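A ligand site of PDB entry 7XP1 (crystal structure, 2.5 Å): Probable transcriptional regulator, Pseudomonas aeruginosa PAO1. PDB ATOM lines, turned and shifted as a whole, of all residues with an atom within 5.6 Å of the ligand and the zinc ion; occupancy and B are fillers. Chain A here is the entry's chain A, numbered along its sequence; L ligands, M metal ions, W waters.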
ATOM      1  N   TYR A  78      10.972  20.982   9.640  1.00  0.00           N
ATOM      2  CA  TYR A  78      11.855  19.841   9.400  1.00  0.00           C
ATOM      3  C   TYR A  78      11.244  18.834   8.427  1.00  0.00           C
ATOM      4  O   TYR A  78      11.989  18.074   7.800  1.00  0.00           O
ATOM      5  CB  TYR A  78      12.193  19.160  10.719  1.00  0.00           C
ATOM      6  CG  TYR A  78      13.451  19.712  11.347  1.00  0.00           C
ATOM      7  CD1 TYR A  78      13.435  20.897  12.063  1.00  0.00           C
ATOM      8  CD2 TYR A  78      14.667  19.048  11.203  1.00  0.00           C
ATOM      9  CE1 TYR A  78      14.582  21.417  12.631  1.00  0.00           C
ATOM     10  CE2 TYR A  78      15.833  19.558  11.766  1.00  0.00           C
ATOM     11  CZ  TYR A  78      15.773  20.743  12.474  1.00  0.00           C
ATOM     12  OH  TYR A  78      16.929  21.253  13.040  1.00  0.00           O
ATOM     13  N   ARG A  81      12.359  20.239   5.144  1.00  0.00           N
ATOM     14  CA  ARG A  81      13.803  20.089   5.066  1.00  0.00           C
ATOM     15  C   ARG A  81      14.203  18.649   4.797  1.00  0.00           C
ATOM     16  O   ARG A  81      15.180  18.393   4.078  1.00  0.00           O
ATOM     17  CB  ARG A  81      14.459  20.594   6.350  1.00  0.00           C
ATOM     18  CG  ARG A  81      15.976  20.536   6.313  1.00  0.00           C
ATOM     19  CD  ARG A  81      16.588  20.920   7.652  1.00  0.00           C
ATOM     20  NE  ARG A  81      18.048  20.811   7.590  1.00  0.00           N
ATOM     21  CZ  ARG A  81      18.827  20.610   8.648  1.00  0.00           C
ATOM     22  NH1 ARG A  81      18.326  20.512   9.869  1.00  0.00           N
ATOM     23  NH2 ARG A  81      20.134  20.488   8.466  1.00  0.00           N
ATOM     24  N   GLN A 126      26.381  25.388  19.612  1.00  0.00           N
ATOM     25  CA  GLN A 126      27.225  24.641  18.693  1.00  0.00           C
ATOM     26  C   GLN A 126      27.347  25.402  17.379  1.00  0.00           C
ATOM     27  O   GLN A 126      26.392  26.055  16.941  1.00  0.00           O
ATOM     28  CB  GLN A 126      26.677  23.231  18.443  1.00  0.00           C
ATOM     29  CG  GLN A 126      27.691  22.275  17.860  1.00  0.00           C
ATOM     30  CD  GLN A 126      27.156  21.492  16.674  1.00  0.00           C
ATOM     31  OE1 GLN A 126      25.963  21.549  16.372  1.00  0.00           O
ATOM     32  NE2 GLN A 126      28.038  20.784  15.985  1.00  0.00           N
ATOM     33  N   GLU A 127      28.519  25.300  16.758  1.00  0.00           N
ATOM     34  CA  GLU A 127      28.755  26.013  15.503  1.00  0.00           C
ATOM     35  C   GLU A 127      27.986  25.374  14.348  1.00  0.00           C
ATOM     36  O   GLU A 127      27.248  26.054  13.633  1.00  0.00           O
ATOM     37  CB  GLU A 127      30.261  26.046  15.196  1.00  0.00           C
ATOM     38  CG  GLU A 127      30.991  24.701  15.223  1.00  0.00           C
ATOM     39  CD  GLU A 127      31.328  24.219  16.626  1.00  0.00           C
ATOM     40  OE1 GLU A 127      30.432  24.185  17.487  1.00  0.00           O
ATOM     41  OE2 GLU A 127      32.507  23.872  16.860  1.00  0.00           O
ATOM     42  N   GLY A 128      28.127  24.068  14.168  1.00  0.00           N
ATOM     43  CA  GLY A 128      27.426  23.340  13.128  1.00  0.00           C
ATOM     44  C   GLY A 128      28.253  23.205  11.859  1.00  0.00           C
ATOM     45  O   GLY A 128      29.305  23.818  11.683  1.00  0.00           O
ATOM     46  N   ASP A 129      27.747  22.360  10.969  1.00  0.00           N
ATOM     47  CA  ASP A 129      28.412  22.082   9.708  1.00  0.00           C
ATOM     48  C   ASP A 129      27.558  22.512   8.527  1.00  0.00           C
ATOM     49  O   ASP A 129      27.260  21.711   7.635  1.00  0.00           O
ATOM     50  CB  ASP A 129      28.749  20.599   9.604  1.00  0.00           C
ATOM     51  CG  ASP A 129      30.092  20.351   8.951  1.00  0.00           C
ATOM     52  OD1 ASP A 129      30.459  21.115   8.022  1.00  0.00           O
ATOM     53  OD2 ASP A 129      30.779  19.382   9.346  1.00  0.00           O
ATOM     54  N   TYR A 130      27.156  23.784   8.504  1.00  0.00           N
ATOM     55  CA  TYR A 130      26.362  24.295   7.388  1.00  0.00           C
ATOM     56  C   TYR A 130      27.098  24.168   6.063  1.00  0.00           C
ATOM     57  O   TYR A 130      26.468  23.992   5.022  1.00  0.00           O
ATOM     58  CB  TYR A 130      25.965  25.745   7.635  1.00  0.00           C
ATOM     59  CG  TYR A 130      25.274  26.399   6.456  1.00  0.00           C
ATOM     60  CD1 TYR A 130      24.095  25.867   5.950  1.00  0.00           C
ATOM     61  CD2 TYR A 130      25.806  27.524   5.853  1.00  0.00           C
ATOM     62  CE1 TYR A 130      23.457  26.451   4.870  1.00  0.00           C
ATOM     63  CE2 TYR A 130      25.177  28.118   4.770  1.00  0.00           C
ATOM     64  CZ  TYR A 130      24.004  27.576   4.284  1.00  0.00           C
ATOM     65  OH  TYR A 130      23.388  28.161   3.207  1.00  0.00           O
ATOM     66  N   PHE A 132      28.935  21.682   5.048  1.00  0.00           N
ATOM     67  CA  PHE A 132      28.687  20.340   4.518  1.00  0.00           C
ATOM     68  C   PHE A 132      27.361  20.277   3.775  1.00  0.00           C
ATOM     69  O   PHE A 132      27.309  19.843   2.619  1.00  0.00           O
ATOM     70  CB  PHE A 132      28.716  19.313   5.660  1.00  0.00           C
ATOM     71  CG  PHE A 132      28.595  17.893   5.195  1.00  0.00           C
ATOM     72  CD1 PHE A 132      29.642  17.269   4.538  1.00  0.00           C
ATOM     73  CD2 PHE A 132      27.424  17.178   5.419  1.00  0.00           C
ATOM     74  CE1 PHE A 132      29.530  15.959   4.112  1.00  0.00           C
ATOM     75  CE2 PHE A 132      27.300  15.867   4.986  1.00  0.00           C
ATOM     76  CZ  PHE A 132      28.359  15.263   4.336  1.00  0.00           C
ATOM     77  N   HIS A 133      26.274  20.711   4.423  1.00  0.00           N
ATOM     78  CA  HIS A 133      24.967  20.698   3.778  1.00  0.00           C
ATOM     79  C   HIS A 133      24.942  21.615   2.572  1.00  0.00           C
ATOM     80  O   HIS A 133      24.301  21.308   1.556  1.00  0.00           O
ATOM     81  CB  HIS A 133      23.885  21.089   4.781  1.00  0.00           C
ATOM     82  CG  HIS A 133      23.619  20.057   5.814  1.00  0.00           C
ATOM     83  ND1 HIS A 133      22.373  19.500   6.009  1.00  0.00           N
ATOM     84  CD2 HIS A 133      24.426  19.468   6.728  1.00  0.00           C
ATOM     85  CE1 HIS A 133      22.422  18.615   6.988  1.00  0.00           C
ATOM     86  NE2 HIS A 133      23.672  18.577   7.441  1.00  0.00           N
ATOM     87  N   TYR A 154      16.501  27.701   5.858  1.00  0.00           N
ATOM     88  CA  TYR A 154      17.638  27.669   6.764  1.00  0.00           C
ATOM     89  C   TYR A 154      17.677  28.854   7.725  1.00  0.00           C
ATOM     90  O   TYR A 154      18.401  28.803   8.716  1.00  0.00           O
ATOM     91  CB  TYR A 154      18.946  27.591   5.975  1.00  0.00           C
ATOM     92  CG  TYR A 154      19.532  26.203   5.941  1.00  0.00           C
ATOM     93  CD1 TYR A 154      20.267  25.712   7.002  1.00  0.00           C
ATOM     94  CD2 TYR A 154      19.329  25.366   4.842  1.00  0.00           C
ATOM     95  CE1 TYR A 154      20.803  24.442   6.984  1.00  0.00           C
ATOM     96  CE2 TYR A 154      19.852  24.086   4.817  1.00  0.00           C
ATOM     97  CZ  TYR A 154      20.589  23.625   5.888  1.00  0.00           C
ATOM     98  OH  TYR A 154      21.116  22.355   5.873  1.00  0.00           O
ATOM     99  N   VAL A 157      15.421  27.580  10.438  1.00  0.00           N
ATOM    100  CA  VAL A 157      16.153  26.491  11.071  1.00  0.00           C
ATOM    101  C   VAL A 157      17.130  27.045  12.109  1.00  0.00           C
ATOM    102  O   VAL A 157      17.206  26.539  13.237  1.00  0.00           O
ATOM    103  CB  VAL A 157      16.901  25.663  10.004  1.00  0.00           C
ATOM    104  CG1 VAL A 157      18.023  24.862  10.632  1.00  0.00           C
ATOM    105  CG2 VAL A 157      15.941  24.748   9.263  1.00  0.00           C
ATOM    106  N   ARG A 161      17.936  26.265  16.308  1.00  0.00           N
ATOM    107  CA  ARG A 161      19.223  25.818  16.854  1.00  0.00           C
ATOM    108  C   ARG A 161      19.877  26.866  17.730  1.00  0.00           C
ATOM    109  O   ARG A 161      20.719  26.518  18.570  1.00  0.00           O
ATOM    110  CB  ARG A 161      20.157  25.434  15.709  1.00  0.00           C
ATOM    111  CG  ARG A 161      20.063  23.974  15.298  1.00  0.00           C
ATOM    112  CD  ARG A 161      21.422  23.301  15.446  1.00  0.00           C
ATOM    113  NE  ARG A 161      22.372  23.847  14.494  1.00  0.00           N
ATOM    114  CZ  ARG A 161      23.687  23.774  14.613  1.00  0.00           C
ATOM    115  NH1 ARG A 161      24.258  23.159  15.641  1.00  0.00           N
ATOM    116  NH2 ARG A 161      24.457  24.325  13.686  1.00  0.00           N
ATOM    117  N   THR A 166      22.325  22.203  21.298  1.00  0.00           N
ATOM    118  CA  THR A 166      22.390  20.755  21.164  1.00  0.00           C
ATOM    119  C   THR A 166      22.955  20.128  22.444  1.00  0.00           C
ATOM    120  O   THR A 166      23.483  20.813  23.328  1.00  0.00           O
ATOM    121  CB  THR A 166      23.245  20.360  19.969  1.00  0.00           C
ATOM    122  OG1 THR A 166      24.483  21.085  19.997  1.00  0.00           O
ATOM    123  CG2 THR A 166      22.523  20.693  18.664  1.00  0.00           C
ATOM    124  N   ARG A 170      25.814  15.508  20.582  1.00  0.00           N
ATOM    125  CA  ARG A 170      25.198  15.743  19.275  1.00  0.00           C
ATOM    126  C   ARG A 170      26.236  16.142  18.223  1.00  0.00           C
ATOM    127  O   ARG A 170      26.150  15.647  17.089  1.00  0.00           O
ATOM    128  CB  ARG A 170      24.098  16.800  19.383  1.00  0.00           C
ATOM    129  CG  ARG A 170      23.292  16.982  18.103  1.00  0.00           C
ATOM    130  CD  ARG A 170      22.781  15.634  17.601  1.00  0.00           C
ATOM    131  NE  ARG A 170      22.370  15.694  16.200  1.00  0.00           N
ATOM    132  CZ  ARG A 170      22.249  14.637  15.422  1.00  0.00           C
ATOM    133  NH1 ARG A 170      22.516  13.419  15.862  1.00  0.00           N
ATOM    134  NH2 ARG A 170      21.857  14.797  14.161  1.00  0.00           N
ATOM    135  N   ALA A 174      26.521  13.879  14.798  1.00  0.00           N
ATOM    136  CA  ALA A 174      26.247  14.422  13.470  1.00  0.00           C
ATOM    137  C   ALA A 174      27.427  14.262  12.532  1.00  0.00           C
ATOM    138  O   ALA A 174      27.234  14.136  11.315  1.00  0.00           O
ATOM    139  CB  ALA A 174      25.850  15.903  13.582  1.00  0.00           C
ATOM    140  N   HIS A 178      27.273  12.621   8.981  1.00  0.00           N
ATOM    141  CA  HIS A 178      27.754  13.338   7.807  1.00  0.00           C
ATOM    142  C   HIS A 178      28.662  12.452   6.953  1.00  0.00           C
ATOM    143  O   HIS A 178      28.574  12.468   5.714  1.00  0.00           O
ATOM    144  CB  HIS A 178      28.483  14.601   8.232  1.00  0.00           C
ATOM    145  CG  HIS A 178      27.581  15.720   8.645  1.00  0.00           C
ATOM    146  ND1 HIS A 178      27.999  16.764   9.437  1.00  0.00           N
ATOM    147  CD2 HIS A 178      26.272  15.945   8.388  1.00  0.00           C
ATOM    148  CE1 HIS A 178      26.987  17.592   9.644  1.00  0.00           C
ATOM    149  NE2 HIS A 178      25.927  17.114   9.018  1.00  0.00           N
ATOM    150  N   HIS A 200      19.433  11.697   9.247  1.00  0.00           N
ATOM    151  CA  HIS A 200      20.206  12.719   9.930  1.00  0.00           C
ATOM    152  C   HIS A 200      19.354  13.960  10.212  1.00  0.00           C
ATOM    153  O   HIS A 200      19.522  14.607  11.249  1.00  0.00           O
ATOM    154  CB  HIS A 200      21.442  13.090   9.110  1.00  0.00           C
ATOM    155  CG  HIS A 200      22.111  14.351   9.542  1.00  0.00           C
ATOM    156  ND1 HIS A 200      22.809  14.458  10.730  1.00  0.00           N
ATOM    157  CD2 HIS A 200      22.185  15.576   8.955  1.00  0.00           C
ATOM    158  CE1 HIS A 200      23.287  15.687  10.844  1.00  0.00           C
ATOM    159  NE2 HIS A 200      22.924  16.377   9.784  1.00  0.00           N
ATOM    160  N   ILE A 201      18.454  14.307   9.286  1.00  0.00           N
ATOM    161  CA  ILE A 201      17.531  15.407   9.528  1.00  0.00           C
ATOM    162  C   ILE A 201      16.593  15.060  10.674  1.00  0.00           C
ATOM    163  O   ILE A 201      16.322  15.889  11.553  1.00  0.00           O
ATOM    164  CB  ILE A 201      16.763  15.759   8.247  1.00  0.00           C
ATOM    165  CG1 ILE A 201      17.710  16.196   7.140  1.00  0.00           C
ATOM    166  CG2 ILE A 201      15.731  16.846   8.512  1.00  0.00           C
ATOM    167  CD1 ILE A 201      18.522  17.410   7.486  1.00  0.00           C
ATOM    168  N   ALA A 203      17.202  12.977  13.113  1.00  0.00           N
ATOM    169  CA  ALA A 203      17.970  13.005  14.352  1.00  0.00           C
ATOM    170  C   ALA A 203      18.141  14.435  14.843  1.00  0.00           C
ATOM    171  O   ALA A 203      18.142  14.678  16.057  1.00  0.00           O
ATOM    172  CB  ALA A 203      19.330  12.344  14.133  1.00  0.00           C
ATOM    173  N   SER A 204      18.276  15.384  13.923  1.00  0.00           N
ATOM    174  CA  SER A 204      18.386  16.784  14.318  1.00  0.00           C
ATOM    175  C   SER A 204      17.096  17.284  14.955  1.00  0.00           C
ATOM    176  O   SER A 204      17.133  18.018  15.948  1.00  0.00           O
ATOM    177  CB  SER A 204      18.758  17.640  13.105  1.00  0.00           C
ATOM    178  OG  SER A 204      18.924  19.001  13.473  1.00  0.00           O
ATOM    179  N   ASN A 207      16.703  15.933  18.445  1.00  0.00           N
ATOM    180  CA  ASN A 207      17.642  16.607  19.338  1.00  0.00           C
ATOM    181  C   ASN A 207      17.079  17.943  19.815  1.00  0.00           C
ATOM    182  O   ASN A 207      17.240  18.319  20.979  1.00  0.00           O
ATOM    183  CB  ASN A 207      18.977  16.819  18.624  1.00  0.00           C
ATOM    184  CG  ASN A 207      20.019  17.455  19.507  1.00  0.00           C
ATOM    185  OD1 ASN A 207      20.288  18.652  19.414  1.00  0.00           O
ATOM    186  ND2 ASN A 207      20.619  16.652  20.379  1.00  0.00           N
ATOM    187  N   ILE A 208      16.401  18.675  18.925  1.00  0.00           N
ATOM    188  CA  ILE A 208      15.781  19.940  19.314  1.00  0.00           C
ATOM    189  C   ILE A 208      14.535  19.688  20.147  1.00  0.00           C
ATOM    190  O   ILE A 208      14.248  20.417  21.104  1.00  0.00           O
ATOM    191  CB  ILE A 208      15.482  20.791  18.067  1.00  0.00           C
ATOM    192  CG1 ILE A 208      16.753  21.451  17.551  1.00  0.00           C
ATOM    193  CG2 ILE A 208      14.422  21.848  18.372  1.00  0.00           C
ATOM    194  CD1 ILE A 208      16.621  22.067  16.179  1.00  0.00           C
HETATM  195  C1  LIG L   1      24.824  20.768  11.146  1.00  0.00           C
HETATM  196  O1  LIG L   1      24.914  21.968  11.495  1.00  0.00           O
HETATM  197  O2  LIG L   1      25.049  20.380   9.978  1.00  0.00           O
HETATM  198  C2  LIG L   1      24.444  19.734  12.183  1.00  0.00           C
HETATM  199  C3  LIG L   1      25.372  19.895  13.373  1.00  0.00           C
HETATM  200  O3  LIG L   1      24.623  18.420  11.647  1.00  0.00           O
HETATM  201  C4  LIG L   1      22.988  19.861  12.662  1.00  0.00           C
HETATM  202  C5  LIG L   1      22.634  18.618  13.462  1.00  0.00           C
HETATM  203  C6  LIG L   1      21.776  18.963  14.646  1.00  0.00           C
HETATM  204  O4  LIG L   1      21.475  20.166  14.843  1.00  0.00           O
HETATM  205  O5  LIG L   1      21.385  18.040  15.384  1.00  0.00           O
HETATM  206  C7  LIG L   1      21.982  20.037  11.549  1.00  0.00           C
HETATM  207  O6  LIG L   1      20.892  20.593  11.821  1.00  0.00           O
HETATM  208  O7  LIG L   1      22.236  19.609  10.404  1.00  0.00           O
HETATM  209 ZN    ZN M   1      24.114  18.352   9.680  1.00  0.00          ZN
HETATM  210  O   HOH W   1      19.722  20.429  16.512  1.00  0.00           O
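The zinc ion is bound by an oxygen (O3) of the ligand, an oxygen (O2) of the ligand, a ring nitrogen (NE2) of His 178, a ring nitrogen (NE2) of His 133, a ring nitrogen (NE2) of His 200 and an oxygen (O7) of the ligand.
The backbone carbonyl oxygen (O) of Ala 174 sits close to a ring nitrogen (ND1) of His 178 (3.3 Å). The guanidinium group of Arg 81 sits close to a ring nitrogen (ND1) of His 133, 3.5 Å away. ND1 of His 133 is in hydrogen-bond range of OH of Tyr 154, 3.1 Å away. OD1 of Asp 129 sits at hydrogen-bond distance from N of Phe 132 (3.4 Å). The guanidinium group (NH2) of Arg 81 lies within hydrogen-bond range of the side-chain hydroxyl (OH) of Tyr 154 (3.3 Å). OG of Ser 204 is in hydrogen-bond range of OH of Tyr 78. The guanidinium group (NH1) of Arg 161 is in hydrogen-bond range of the side-chain amide oxygen (OE1) of Gln 126 (2.5 Å). The guanidinium group (NH2) of Arg 161 lies within hydrogen-bond range of the backbone carbonyl oxygen (O) of Glu 127.
Gln 126 touches the ligand (OE1 to C3, 3.5 Å). Gly 128 touches the ligand (CA to O1, 3.3 Å). Thr 166 touches the ligand. CB of Ala 174 touches O3 of the ligand, 3.4 Å away. Hydrophobic or aromatic side chains within 4 Å of the ligand: His 133, Ala 174, His 178 and His 200. Of the 22 residues printed, 12 come within 4 Å of the ligand.
An oxygen (O5) of the ligand is in salt-bridge range of the guanidinium group (NE) of Arg 170 (2.7 Å). N of Asp 129 sits at hydrogen-bond distance from O1 of the ligand (2.9 Å). NH1 of Arg 81 lies within salt-bridge range of O6 of the ligand (3.2 Å). O6 of the ligand lies within hydrogen-bond range of OG of Ser 204, 3.0 Å away. NH2 of Arg 161 lies within salt-bridge range of O1 of the ligand (3.3 Å).
Water W1 lies within hydrogen-bond range of O4 of the ligand, OD1 of Asn 207 and OG of Ser 204.
Of the 22 residues printed, 3 come within 4 Å of the zinc ion. The nearest printed residue that does not touch the zinc ion is Arg 81 (4.7 Å).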
